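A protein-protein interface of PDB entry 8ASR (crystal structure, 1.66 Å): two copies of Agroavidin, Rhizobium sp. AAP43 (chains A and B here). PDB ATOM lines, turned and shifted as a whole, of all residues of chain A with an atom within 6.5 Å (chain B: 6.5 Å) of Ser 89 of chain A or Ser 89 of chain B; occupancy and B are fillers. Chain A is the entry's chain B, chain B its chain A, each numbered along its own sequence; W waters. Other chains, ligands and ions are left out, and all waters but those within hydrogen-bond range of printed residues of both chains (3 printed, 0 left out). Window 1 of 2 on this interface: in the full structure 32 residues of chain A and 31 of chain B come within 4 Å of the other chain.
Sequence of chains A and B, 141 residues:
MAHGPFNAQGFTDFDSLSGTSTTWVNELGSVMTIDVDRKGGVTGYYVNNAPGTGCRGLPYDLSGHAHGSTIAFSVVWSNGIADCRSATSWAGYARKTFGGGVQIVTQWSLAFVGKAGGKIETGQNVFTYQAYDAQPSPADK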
ATOM      1  N   ILE A  71      17.726  32.569  26.502  1.00  0.00           N
ATOM      2  CA  ILE A  71      18.222  31.386  27.233  1.00  0.00           C
ATOM      3  C   ILE A  71      17.823  30.138  26.460  1.00  0.00           C
ATOM      4  O   ILE A  71      16.811  30.133  25.754  1.00  0.00           O
ATOM      5  CB  ILE A  71      17.744  31.378  28.692  1.00  0.00           C
ATOM      6  CG1 ILE A  71      18.399  30.255  29.504  1.00  0.00           C
ATOM      7  CG2 ILE A  71      16.225  31.326  28.739  1.00  0.00           C
ATOM      8  CD1 ILE A  71      18.084  30.315  30.953  1.00  0.00           C
ATOM      9  N   ALA A  72      18.640  29.090  26.583  1.00  0.00           N
ATOM     10  CA  ALA A  72      18.283  27.785  25.998  1.00  0.00           C
ATOM     11  C   ALA A  72      18.870  26.692  26.866  1.00  0.00           C
ATOM     12  O   ALA A  72      19.964  26.927  27.465  1.00  0.00           O
ATOM     13  CB  ALA A  72      18.741  27.679  24.566  1.00  0.00           C
ATOM     14  N   PHE A  73      18.160  25.575  26.978  1.00  0.00           N
ATOM     15  CA  PHE A  73      18.605  24.452  27.820  1.00  0.00           C
ATOM     16  C   PHE A  73      18.003  23.154  27.307  1.00  0.00           C
ATOM     17  O   PHE A  73      16.971  23.182  26.619  1.00  0.00           O
ATOM     18  CB  PHE A  73      18.419  24.746  29.305  1.00  0.00           C
ATOM     19  CG  PHE A  73      17.005  25.168  29.630  1.00  0.00           C
ATOM     20  CD1 PHE A  73      16.046  24.220  29.938  1.00  0.00           C
ATOM     21  CD2 PHE A  73      16.669  26.499  29.675  1.00  0.00           C
ATOM     22  CE1 PHE A  73      14.757  24.609  30.286  1.00  0.00           C
ATOM     23  CE2 PHE A  73      15.364  26.881  29.932  1.00  0.00           C
ATOM     24  CZ  PHE A  73      14.417  25.930  30.237  1.00  0.00           C
ATOM     25  N   SER A  74      18.638  22.035  27.676  1.00  0.00           N
ATOM     26  CA  SER A  74      18.339  20.695  27.135  1.00  0.00           C
ATOM     27  C   SER A  74      18.340  19.678  28.276  1.00  0.00           C
ATOM     28  O   SER A  74      19.136  19.826  29.216  1.00  0.00           O
ATOM     29  CB  SER A  74      19.367  20.330  26.076  1.00  0.00           C
ATOM     30  OG  SER A  74      19.296  21.284  25.001  1.00  0.00           O
ATOM     31  N   VAL A  75      17.511  18.656  28.122  1.00  0.00           N
ATOM     32  CA  VAL A  75      17.399  17.478  29.020  1.00  0.00           C
ATOM     33  C   VAL A  75      17.216  16.259  28.124  1.00  0.00           C
ATOM     34  O   VAL A  75      16.374  16.314  27.240  1.00  0.00           O
ATOM     35  CB  VAL A  75      16.170  17.649  29.948  1.00  0.00           C
ATOM     36  CG1 VAL A  75      15.874  16.353  30.677  1.00  0.00           C
ATOM     37  CG2 VAL A  75      16.381  18.769  30.930  1.00  0.00           C
ATOM     38  N   ALA A  87      13.850  13.226  24.472  1.00  0.00           N
ATOM     39  CA  ALA A  87      14.692  14.394  24.794  1.00  0.00           C
ATOM     40  C   ALA A  87      13.881  15.677  24.622  1.00  0.00           C
ATOM     41  O   ALA A  87      13.083  15.788  23.694  1.00  0.00           O
ATOM     42  CB  ALA A  87      15.943  14.407  23.935  1.00  0.00           C
ATOM     43  N   THR A  88      14.154  16.692  25.434  1.00  0.00           N
ATOM     44  CA  THR A  88      13.459  17.988  25.326  1.00  0.00           C
ATOM     45  C   THR A  88      14.486  19.107  25.347  1.00  0.00           C
ATOM     46  O   THR A  88      15.413  19.047  26.162  1.00  0.00           O
ATOM     47  CB  THR A  88      12.391  18.165  26.425  1.00  0.00           C
ATOM     48  OG1 THR A  88      11.516  17.026  26.364  1.00  0.00           O
ATOM     49  CG2 THR A  88      11.571  19.425  26.240  1.00  0.00           C
ATOM     50  N   SER A  89      14.251  20.141  24.544  1.00  0.00           N
ATOM     51  CA  SER A  89      15.026  21.397  24.571  1.00  0.00           C
ATOM     52  C   SER A  89      14.066  22.573  24.649  1.00  0.00           C
ATOM     53  O   SER A  89      12.989  22.440  24.082  1.00  0.00           O
ATOM     54  CB  SER A  89      15.929  21.490  23.345  1.00  0.00           C
ATOM     55  OG  SER A  89      16.982  22.404  23.582  1.00  0.00           O
ATOM     56  N   TRP A  90      14.509  23.640  25.292  1.00  0.00           N
ATOM     57  CA  TRP A  90      13.762  24.886  25.450  1.00  0.00           C
ATOM     58  C   TRP A  90      14.605  26.037  24.917  1.00  0.00           C
ATOM     59  O   TRP A  90      15.821  26.049  25.147  1.00  0.00           O
ATOM     60  CB  TRP A  90      13.437  25.089  26.914  1.00  0.00           C
ATOM     61  CG  TRP A  90      12.466  24.151  27.565  1.00  0.00           C
ATOM     62  CD1 TRP A  90      11.147  24.404  27.855  1.00  0.00           C
ATOM     63  CD2 TRP A  90      12.769  22.874  28.135  1.00  0.00           C
ATOM     64  NE1 TRP A  90      10.609  23.364  28.550  1.00  0.00           N
ATOM     65  CE2 TRP A  90      11.589  22.426  28.766  1.00  0.00           C
ATOM     66  CE3 TRP A  90      13.944  22.104  28.227  1.00  0.00           C
ATOM     67  CZ2 TRP A  90      11.535  21.199  29.400  1.00  0.00           C
ATOM     68  CZ3 TRP A  90      13.895  20.893  28.883  1.00  0.00           C
ATOM     69  CH2 TRP A  90      12.702  20.473  29.505  1.00  0.00           C
ATOM     70  N   ALA A  91      13.959  26.977  24.223  1.00  0.00           N
ATOM     71  CA  ALA A  91      14.583  28.280  23.939  1.00  0.00           C
ATOM     72  C   ALA A  91      13.604  29.313  24.422  1.00  0.00           C
ATOM     73  O   ALA A  91      12.420  29.086  24.217  1.00  0.00           O
ATOM     74  CB  ALA A  91      14.863  28.433  22.443  1.00  0.00           C
ATOM     75  N   GLN A 107       9.614  28.051  24.187  1.00  0.00           N
ATOM     76  CA  GLN A 107       9.035  27.010  23.315  1.00  0.00           C
ATOM     77  C   GLN A 107       9.909  25.789  23.506  1.00  0.00           C
ATOM     78  O   GLN A 107      11.163  25.951  23.439  1.00  0.00           O
ATOM     79  CB  GLN A 107       9.012  27.501  21.870  1.00  0.00           C
ATOM     80  CG  GLN A 107       8.273  26.626  20.873  1.00  0.00           C
ATOM     81  CD  GLN A 107       6.793  26.950  20.848  1.00  0.00           C
ATOM     82  OE1 GLN A 107       6.363  27.950  21.404  1.00  0.00           O
ATOM     83  NE2 GLN A 107       6.005  26.069  20.271  1.00  0.00           N
ATOM     84  N   TRP A 108       9.283  24.656  23.759  1.00  0.00           N
ATOM     85  CA  TRP A 108       9.993  23.366  23.890  1.00  0.00           C
ATOM     86  C   TRP A 108       9.859  22.587  22.583  1.00  0.00           C
ATOM     87  O   TRP A 108       8.856  22.789  21.851  1.00  0.00           O
ATOM     88  CB  TRP A 108       9.501  22.566  25.080  1.00  0.00           C
ATOM     89  CG  TRP A 108       8.031  22.370  25.213  1.00  0.00           C
ATOM     90  CD1 TRP A 108       7.169  23.058  26.022  1.00  0.00           C
ATOM     91  CD2 TRP A 108       7.260  21.361  24.543  1.00  0.00           C
ATOM     92  NE1 TRP A 108       5.918  22.546  25.900  1.00  0.00           N
ATOM     93  CE2 TRP A 108       5.932  21.512  24.991  1.00  0.00           C
ATOM     94  CE3 TRP A 108       7.559  20.394  23.581  1.00  0.00           C
ATOM     95  CZ2 TRP A 108       4.915  20.682  24.523  1.00  0.00           C
ATOM     96  CZ3 TRP A 108       6.552  19.579  23.109  1.00  0.00           C
ATOM     97  CH2 TRP A 108       5.242  19.724  23.596  1.00  0.00           C
ATOM     98  N   SER A 109      10.901  21.807  22.296  1.00  0.00           N
ATOM     99  CA  SER A 109      11.006  20.831  21.188  1.00  0.00           C
ATOM    100  C   SER A 109      11.135  19.477  21.876  1.00  0.00           C
ATOM    101  O   SER A 109      11.992  19.347  22.793  1.00  0.00           O
ATOM    102  CB  SER A 109      12.170  21.157  20.305  1.00  0.00           C
ATOM    103  OG  SER A 109      12.083  22.494  19.793  1.00  0.00           O
ATOM    104  N   LEU A 110      10.318  18.520  21.480  1.00  0.00           N
ATOM    105  CA  LEU A 110      10.348  17.167  22.089  1.00  0.00           C
ATOM    106  C   LEU A 110      10.558  16.158  20.978  1.00  0.00           C
ATOM    107  O   LEU A 110       9.901  16.285  19.923  1.00  0.00           O
ATOM    108  CB  LEU A 110       9.058  16.942  22.868  1.00  0.00           C
ATOM    109  CG  LEU A 110       8.727  15.501  23.262  1.00  0.00           C
ATOM    110  CD1 LEU A 110       9.558  14.991  24.428  1.00  0.00           C
ATOM    111  CD2 LEU A 110       7.246  15.361  23.601  1.00  0.00           C
ATOM    112  N   SER B  63      25.716  22.933  23.667  1.00  0.00           N
ATOM    113  CA  SER B  63      25.634  21.957  24.771  1.00  0.00           C
ATOM    114  C   SER B  63      24.320  21.200  24.686  1.00  0.00           C
ATOM    115  O   SER B  63      23.345  21.736  24.157  1.00  0.00           O
ATOM    116  CB  SER B  63      25.760  22.625  26.150  1.00  0.00           C
ATOM    117  OG  SER B  63      24.655  23.457  26.428  1.00  0.00           O
ATOM    118  N   ALA B  72      19.063  16.279  22.557  1.00  0.00           N
ATOM    119  CA  ALA B  72      18.568  17.667  22.679  1.00  0.00           C
ATOM    120  C   ALA B  72      19.796  18.530  22.851  1.00  0.00           C
ATOM    121  O   ALA B  72      20.707  18.072  23.563  1.00  0.00           O
ATOM    122  CB  ALA B  72      17.601  17.843  23.836  1.00  0.00           C
ATOM    123  N   PHE B  73      19.863  19.674  22.187  1.00  0.00           N
ATOM    124  CA  PHE B  73      21.047  20.534  22.288  1.00  0.00           C
ATOM    125  C   PHE B  73      20.638  21.946  21.963  1.00  0.00           C
ATOM    126  O   PHE B  73      19.551  22.201  21.373  1.00  0.00           O
ATOM    127  CB  PHE B  73      22.178  20.030  21.388  1.00  0.00           C
ATOM    128  CG  PHE B  73      21.847  19.949  19.929  1.00  0.00           C
ATOM    129  CD1 PHE B  73      21.361  18.777  19.373  1.00  0.00           C
ATOM    130  CD2 PHE B  73      22.148  21.002  19.078  1.00  0.00           C
ATOM    131  CE1 PHE B  73      21.086  18.705  18.009  1.00  0.00           C
ATOM    132  CE2 PHE B  73      21.882  20.924  17.719  1.00  0.00           C
ATOM    133  CZ  PHE B  73      21.350  19.780  17.186  1.00  0.00           C
ATOM    134  N   SER B  74      21.494  22.866  22.378  1.00  0.00           N
ATOM    135  CA  SER B  74      21.185  24.286  22.151  1.00  0.00           C
ATOM    136  C   SER B  74      22.453  25.078  21.903  1.00  0.00           C
ATOM    137  O   SER B  74      23.566  24.593  22.219  1.00  0.00           O
ATOM    138  CB  SER B  74      20.400  24.843  23.250  1.00  0.00           C
ATOM    139  OG  SER B  74      21.185  25.073  24.403  1.00  0.00           O
ATOM    140  N   VAL B  75      22.253  26.216  21.268  1.00  0.00           N
ATOM    141  CA  VAL B  75      23.342  27.171  20.907  1.00  0.00           C
ATOM    142  C   VAL B  75      22.832  28.584  21.213  1.00  0.00           C
ATOM    143  O   VAL B  75      21.803  28.986  20.674  1.00  0.00           O
ATOM    144  CB  VAL B  75      23.732  27.052  19.417  1.00  0.00           C
ATOM    145  CG1 VAL B  75      24.694  28.186  19.014  1.00  0.00           C
ATOM    146  CG2 VAL B  75      24.302  25.682  19.054  1.00  0.00           C
ATOM    147  N   ALA B  87      18.987  32.607  20.646  1.00  0.00           N
ATOM    148  CA  ALA B  87      19.310  31.231  21.074  1.00  0.00           C
ATOM    149  C   ALA B  87      18.436  30.276  20.278  1.00  0.00           C
ATOM    150  O   ALA B  87      17.236  30.500  20.135  1.00  0.00           O
ATOM    151  CB  ALA B  87      19.076  31.070  22.544  1.00  0.00           C
ATOM    152  N   THR B  88      19.007  29.157  19.876  1.00  0.00           N
ATOM    153  CA  THR B  88      18.271  28.100  19.185  1.00  0.00           C
ATOM    154  C   THR B  88      18.413  26.824  20.005  1.00  0.00           C
ATOM    155  O   THR B  88      19.533  26.549  20.554  1.00  0.00           O
ATOM    156  CB  THR B  88      18.825  27.848  17.782  1.00  0.00           C
ATOM    157  OG1 THR B  88      18.752  29.090  17.080  1.00  0.00           O
ATOM    158  CG2 THR B  88      18.019  26.790  17.069  1.00  0.00           C
ATOM    159  N   SER B  89      17.338  26.062  20.073  1.00  0.00           N
ATOM    160  CA  SER B  89      17.379  24.745  20.738  1.00  0.00           C
ATOM    161  C   SER B  89      16.738  23.721  19.817  1.00  0.00           C
ATOM    162  O   SER B  89      15.766  24.064  19.081  1.00  0.00           O
ATOM    163  CB  SER B  89      16.721  24.819  22.107  1.00  0.00           C
ATOM    164  OG  SER B  89      15.399  24.356  22.126  1.00  0.00           O
ATOM    165  N   TRP B  90      17.272  22.522  19.842  1.00  0.00           N
ATOM    166  CA  TRP B  90      16.826  21.396  18.978  1.00  0.00           C
ATOM    167  C   TRP B  90      16.505  20.182  19.862  1.00  0.00           C
ATOM    168  O   TRP B  90      17.173  19.940  20.900  1.00  0.00           O
ATOM    169  CB  TRP B  90      17.925  20.991  17.974  1.00  0.00           C
ATOM    170  CG  TRP B  90      18.360  21.948  16.904  1.00  0.00           C
ATOM    171  CD1 TRP B  90      18.076  21.854  15.574  1.00  0.00           C
ATOM    172  CD2 TRP B  90      19.304  23.014  17.024  1.00  0.00           C
ATOM    173  NE1 TRP B  90      18.729  22.842  14.865  1.00  0.00           N
ATOM    174  CE2 TRP B  90      19.487  23.567  15.738  1.00  0.00           C
ATOM    175  CE3 TRP B  90      20.018  23.576  18.087  1.00  0.00           C
ATOM    176  CZ2 TRP B  90      20.347  24.637  15.510  1.00  0.00           C
ATOM    177  CZ3 TRP B  90      20.856  24.642  17.863  1.00  0.00           C
ATOM    178  CH2 TRP B  90      21.018  25.160  16.586  1.00  0.00           C
ATOM    179  N   ALA B  91      15.628  19.326  19.367  1.00  0.00           N
ATOM    180  CA  ALA B  91      15.421  17.968  19.885  1.00  0.00           C
ATOM    181  C   ALA B  91      15.178  17.080  18.686  1.00  0.00           C
ATOM    182  O   ALA B  91      14.506  17.495  17.760  1.00  0.00           O
ATOM    183  CB  ALA B  91      14.248  17.927  20.819  1.00  0.00           C
ATOM    184  N   GLN B 107      13.428  19.017  15.552  1.00  0.00           N
ATOM    185  CA  GLN B 107      12.512  20.167  15.658  1.00  0.00           C
ATOM    186  C   GLN B 107      13.296  21.260  16.380  1.00  0.00           C
ATOM    187  O   GLN B 107      14.053  20.929  17.309  1.00  0.00           O
ATOM    188  CB  GLN B 107      11.303  19.745  16.475  1.00  0.00           C
ATOM    189  CG  GLN B 107      10.387  20.878  16.882  1.00  0.00           C
ATOM    190  CD  GLN B 107       9.560  21.511  15.808  1.00  0.00           C
ATOM    191  OE1 GLN B 107       9.213  22.703  15.896  1.00  0.00           O
ATOM    192  NE2 GLN B 107       9.136  20.698  14.849  1.00  0.00           N
ATOM    193  N   TRP B 108      13.192  22.520  15.966  1.00  0.00           N
ATOM    194  CA  TRP B 108      13.964  23.580  16.654  1.00  0.00           C
ATOM    195  C   TRP B 108      13.088  24.788  16.970  1.00  0.00           C
ATOM    196  O   TRP B 108      12.037  24.987  16.299  1.00  0.00           O
ATOM    197  CB  TRP B 108      15.204  23.979  15.841  1.00  0.00           C
ATOM    198  CG  TRP B 108      14.946  24.444  14.440  1.00  0.00           C
ATOM    199  CD1 TRP B 108      15.080  23.724  13.288  1.00  0.00           C
ATOM    200  CD2 TRP B 108      14.440  25.733  14.043  1.00  0.00           C
ATOM    201  NE1 TRP B 108      14.726  24.482  12.200  1.00  0.00           N
ATOM    202  CE2 TRP B 108      14.356  25.727  12.634  1.00  0.00           C
ATOM    203  CE3 TRP B 108      14.151  26.913  14.727  1.00  0.00           C
ATOM    204  CZ2 TRP B 108      13.938  26.843  11.919  1.00  0.00           C
ATOM    205  CZ3 TRP B 108      13.756  28.034  14.014  1.00  0.00           C
ATOM    206  CH2 TRP B 108      13.629  27.982  12.626  1.00  0.00           C
ATOM    207  N   SER B 109      13.558  25.567  17.947  1.00  0.00           N
ATOM    208  CA  SER B 109      13.035  26.917  18.261  1.00  0.00           C
ATOM    209  C   SER B 109      14.172  27.901  18.301  1.00  0.00           C
ATOM    210  O   SER B 109      15.238  27.526  18.783  1.00  0.00           O
ATOM    211  CB  SER B 109      12.339  26.946  19.568  1.00  0.00           C
ATOM    212  OG  SER B 109      11.410  25.894  19.605  1.00  0.00           O
ATOM    213  N   LEU B 110      13.912  29.093  17.795  1.00  0.00           N
ATOM    214  CA  LEU B 110      14.823  30.251  17.847  1.00  0.00           C
ATOM    215  C   LEU B 110      14.133  31.324  18.673  1.00  0.00           C
ATOM    216  O   LEU B 110      13.003  31.772  18.259  1.00  0.00           O
ATOM    217  CB  LEU B 110      15.125  30.754  16.443  1.00  0.00           C
ATOM    218  CG  LEU B 110      15.730  32.159  16.379  1.00  0.00           C
ATOM    219  CD1 LEU B 110      17.180  32.130  16.826  1.00  0.00           C
ATOM    220  CD2 LEU B 110      15.641  32.695  14.954  1.00  0.00           C
ATOM    221  N   ALA B 111      14.739  31.721  19.788  1.00  0.00           N
ATOM    222  CA  ALA B 111      14.253  32.837  20.628  1.00  0.00           C
ATOM    223  C   ALA B 111      15.088  34.068  20.336  1.00  0.00           C
ATOM    224  O   ALA B 111      16.300  33.942  20.263  1.00  0.00           O
ATOM    225  CB  ALA B 111      14.278  32.482  22.102  1.00  0.00           C
HETATM  226  O   HOH W   1       9.920  23.828  18.549  1.00  0.00           O
HETATM  227  O   HOH W   2      21.356  22.722  25.824  1.00  0.00           O
HETATM  228  O   HOH W   3      12.845  24.449  21.508  1.00  0.00           O
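N of Trp 90 of chain B sits at hydrogen-bond distance from O of Phe 73 of chain B, at 2.8 Å.
The backbone NH (N) of Ala 111 of chain B lies within hydrogen-bond range of the backbone carbonyl oxygen (O) of Ala 87 of chain B (2.8 Å).
The backbone carbonyl oxygen (O) of Ala 91 of chain B lies within hydrogen-bond range of the backbone NH (N) of Gln 107 of chain B (2.9 Å).
The side-chain hydroxyl (OG) of Ser 89 of chain A is in hydrogen-bond range of the backbone carbonyl oxygen (O) of Phe 73 of chain A (3.1 Å).
O of Phe 73 of chain A lies within hydrogen-bond range of N of Trp 90 of chain A (2.8 Å).
N of Ser 109 of chain A is in hydrogen-bond range of O of Ser 89 of chain A.
Of the 14 printed residues of chain A, 10 touch a printed residue of chain B.
Hydrophobic or aromatic side chains of chain A within 4 Å of the printed part of chain B: Ala 72, Ala 87 and Ala 91.
Among the printed residues, 22 pairs touch across the chains.
Among the printed residues, no Asp or Glu carboxylate lies within 4 Å of a Lys or Arg side-chain nitrogen of the other chain.
The backbone NH of Phe 73 of chain B lies within hydrogen-bond range of the side-chain hydroxyl of Ser 74 of chain A.
O of Phe 73 of chain B lies within hydrogen-bond range of OG of Ser 89 of chain A, at 3.4 Å.
The side-chain hydroxyl (OG) of Ser 89 of chain B sits close to the side-chain hydroxyl (OG) of Ser 89 of chain A.
OG of Ser 89 of chain B lies close to N of Trp 90 of chain A, at 3.4 Å.
OG of Ser 109 of chain B lies within hydrogen-bond range of OG of Ser 109 of chain A (3.5 Å).
Ser 74 of chain A touches its own counterpart, Ser 74 of chain B.
Ser 89 of chain A touches Phe 73 of chain B, but with the chains exchanged Phe 73 of chain A does not touch Ser 89 of chain B (4.8 Å).
Ser 89 of chain A touches Trp 90 of chain B, and with the chains exchanged Trp 90 of chain A touches Ser 89 of chain B.
Ala 91 of chain A touches Ser 109 of chain B, and with the chains exchanged Ser 109 of chain A touches Ala 91 of chain B.
13 positions are printed for both chains.
Water W3 lies within hydrogen-bond range of the side-chain hydroxyl of Ser 89 of chain B, the side-chain hydroxyl of Ser 109 of chain A, the side-chain hydroxyl of Ser 109 of chain B, the backbone carbonyl oxygen of Gln 107 of chain A and the backbone carbonyl oxygen of Ser 89 of chain A.
Water W2 lies within hydrogen-bond range of the side-chain hydroxyl (OG) of Ser 74 of chain A (2.6 Å), the side-chain hydroxyl (OG) of Ser 74 of chain B (2.8 Å) and the backbone carbonyl oxygen (O) of Ser 63 of chain B (2.8 Å).
Water W1 lies within hydrogen-bond range of the side-chain hydroxyl of Ser 109 of chain B (2.8 Å), the side-chain hydroxyl of Ser 109 of chain A (2.8 Å), the side-chain amide oxygen of Gln 107 of chain B (3.0 Å) and the backbone carbonyl oxygen of Trp 108 of chain B (3.3 Å).
Among the printed residues, merely in contact across the chains: Ala 72 of chain A with Ser 74 of chain B (3.5 Å), Ala 72 of chain A with Ala 87 of chain B (3.96 Å), Ser 74 of chain A with Ala 72 of chain B (3.5 Å), Ser 74 of chain A with Ser 74 of chain B (3.8 Å), Val 75 of chain A with Ala 72 of chain B (3.9 Å), Ala 87 of chain A with Ala 72 of chain B (3.8 Å), Ala 87 of chain A with Ala 91 of chain B (3.8 Å), Thr 88 of chain A with Ala 72 of chain B (3.4 Å), Ser 89 of chain A with Trp 90 of chain B (3.2 Å), Ala 91 of chain A with Ala 87 of chain B (3.9 Å), Ala 91 of chain A with Ser 89 of chain B (3.7 Å), Ala 91 of chain A with Ser 109 of chain B (3.8 Å), Ala 91 of chain A with Ala 111 of chain B (3.98 Å), Gln 107 of chain A with Ser 109 of chain B (3.5 Å), Ser 109 of chain A with Ala 91 of chain B (3.3 Å), Ser 109 of chain A with Gln 107 of chain B (3.5 Å) and Ser 109 of chain A with Trp 108 of chain B (3.8 Å).
Phe 73 of chain A touches none of the printed residues of chain B.
Of the printed residues of chain B, Ser 89 of chain A touches Phe 73, Ser 89 and Trp 90.
Of the printed residues of chain B, Ala 91 of chain A touches Ala 87, Ser 89, Ser 109 and Ala 111.
Leu 110 of chain A touches none of the printed residues of chain B.
Printed residues of chain A within 4 Å of Ala 111 of chain B: Ala 91.
The nearest printed residue of chain B that does not touch Ser 89 of chain A is Ala 72 of chain B (4.04 Å).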
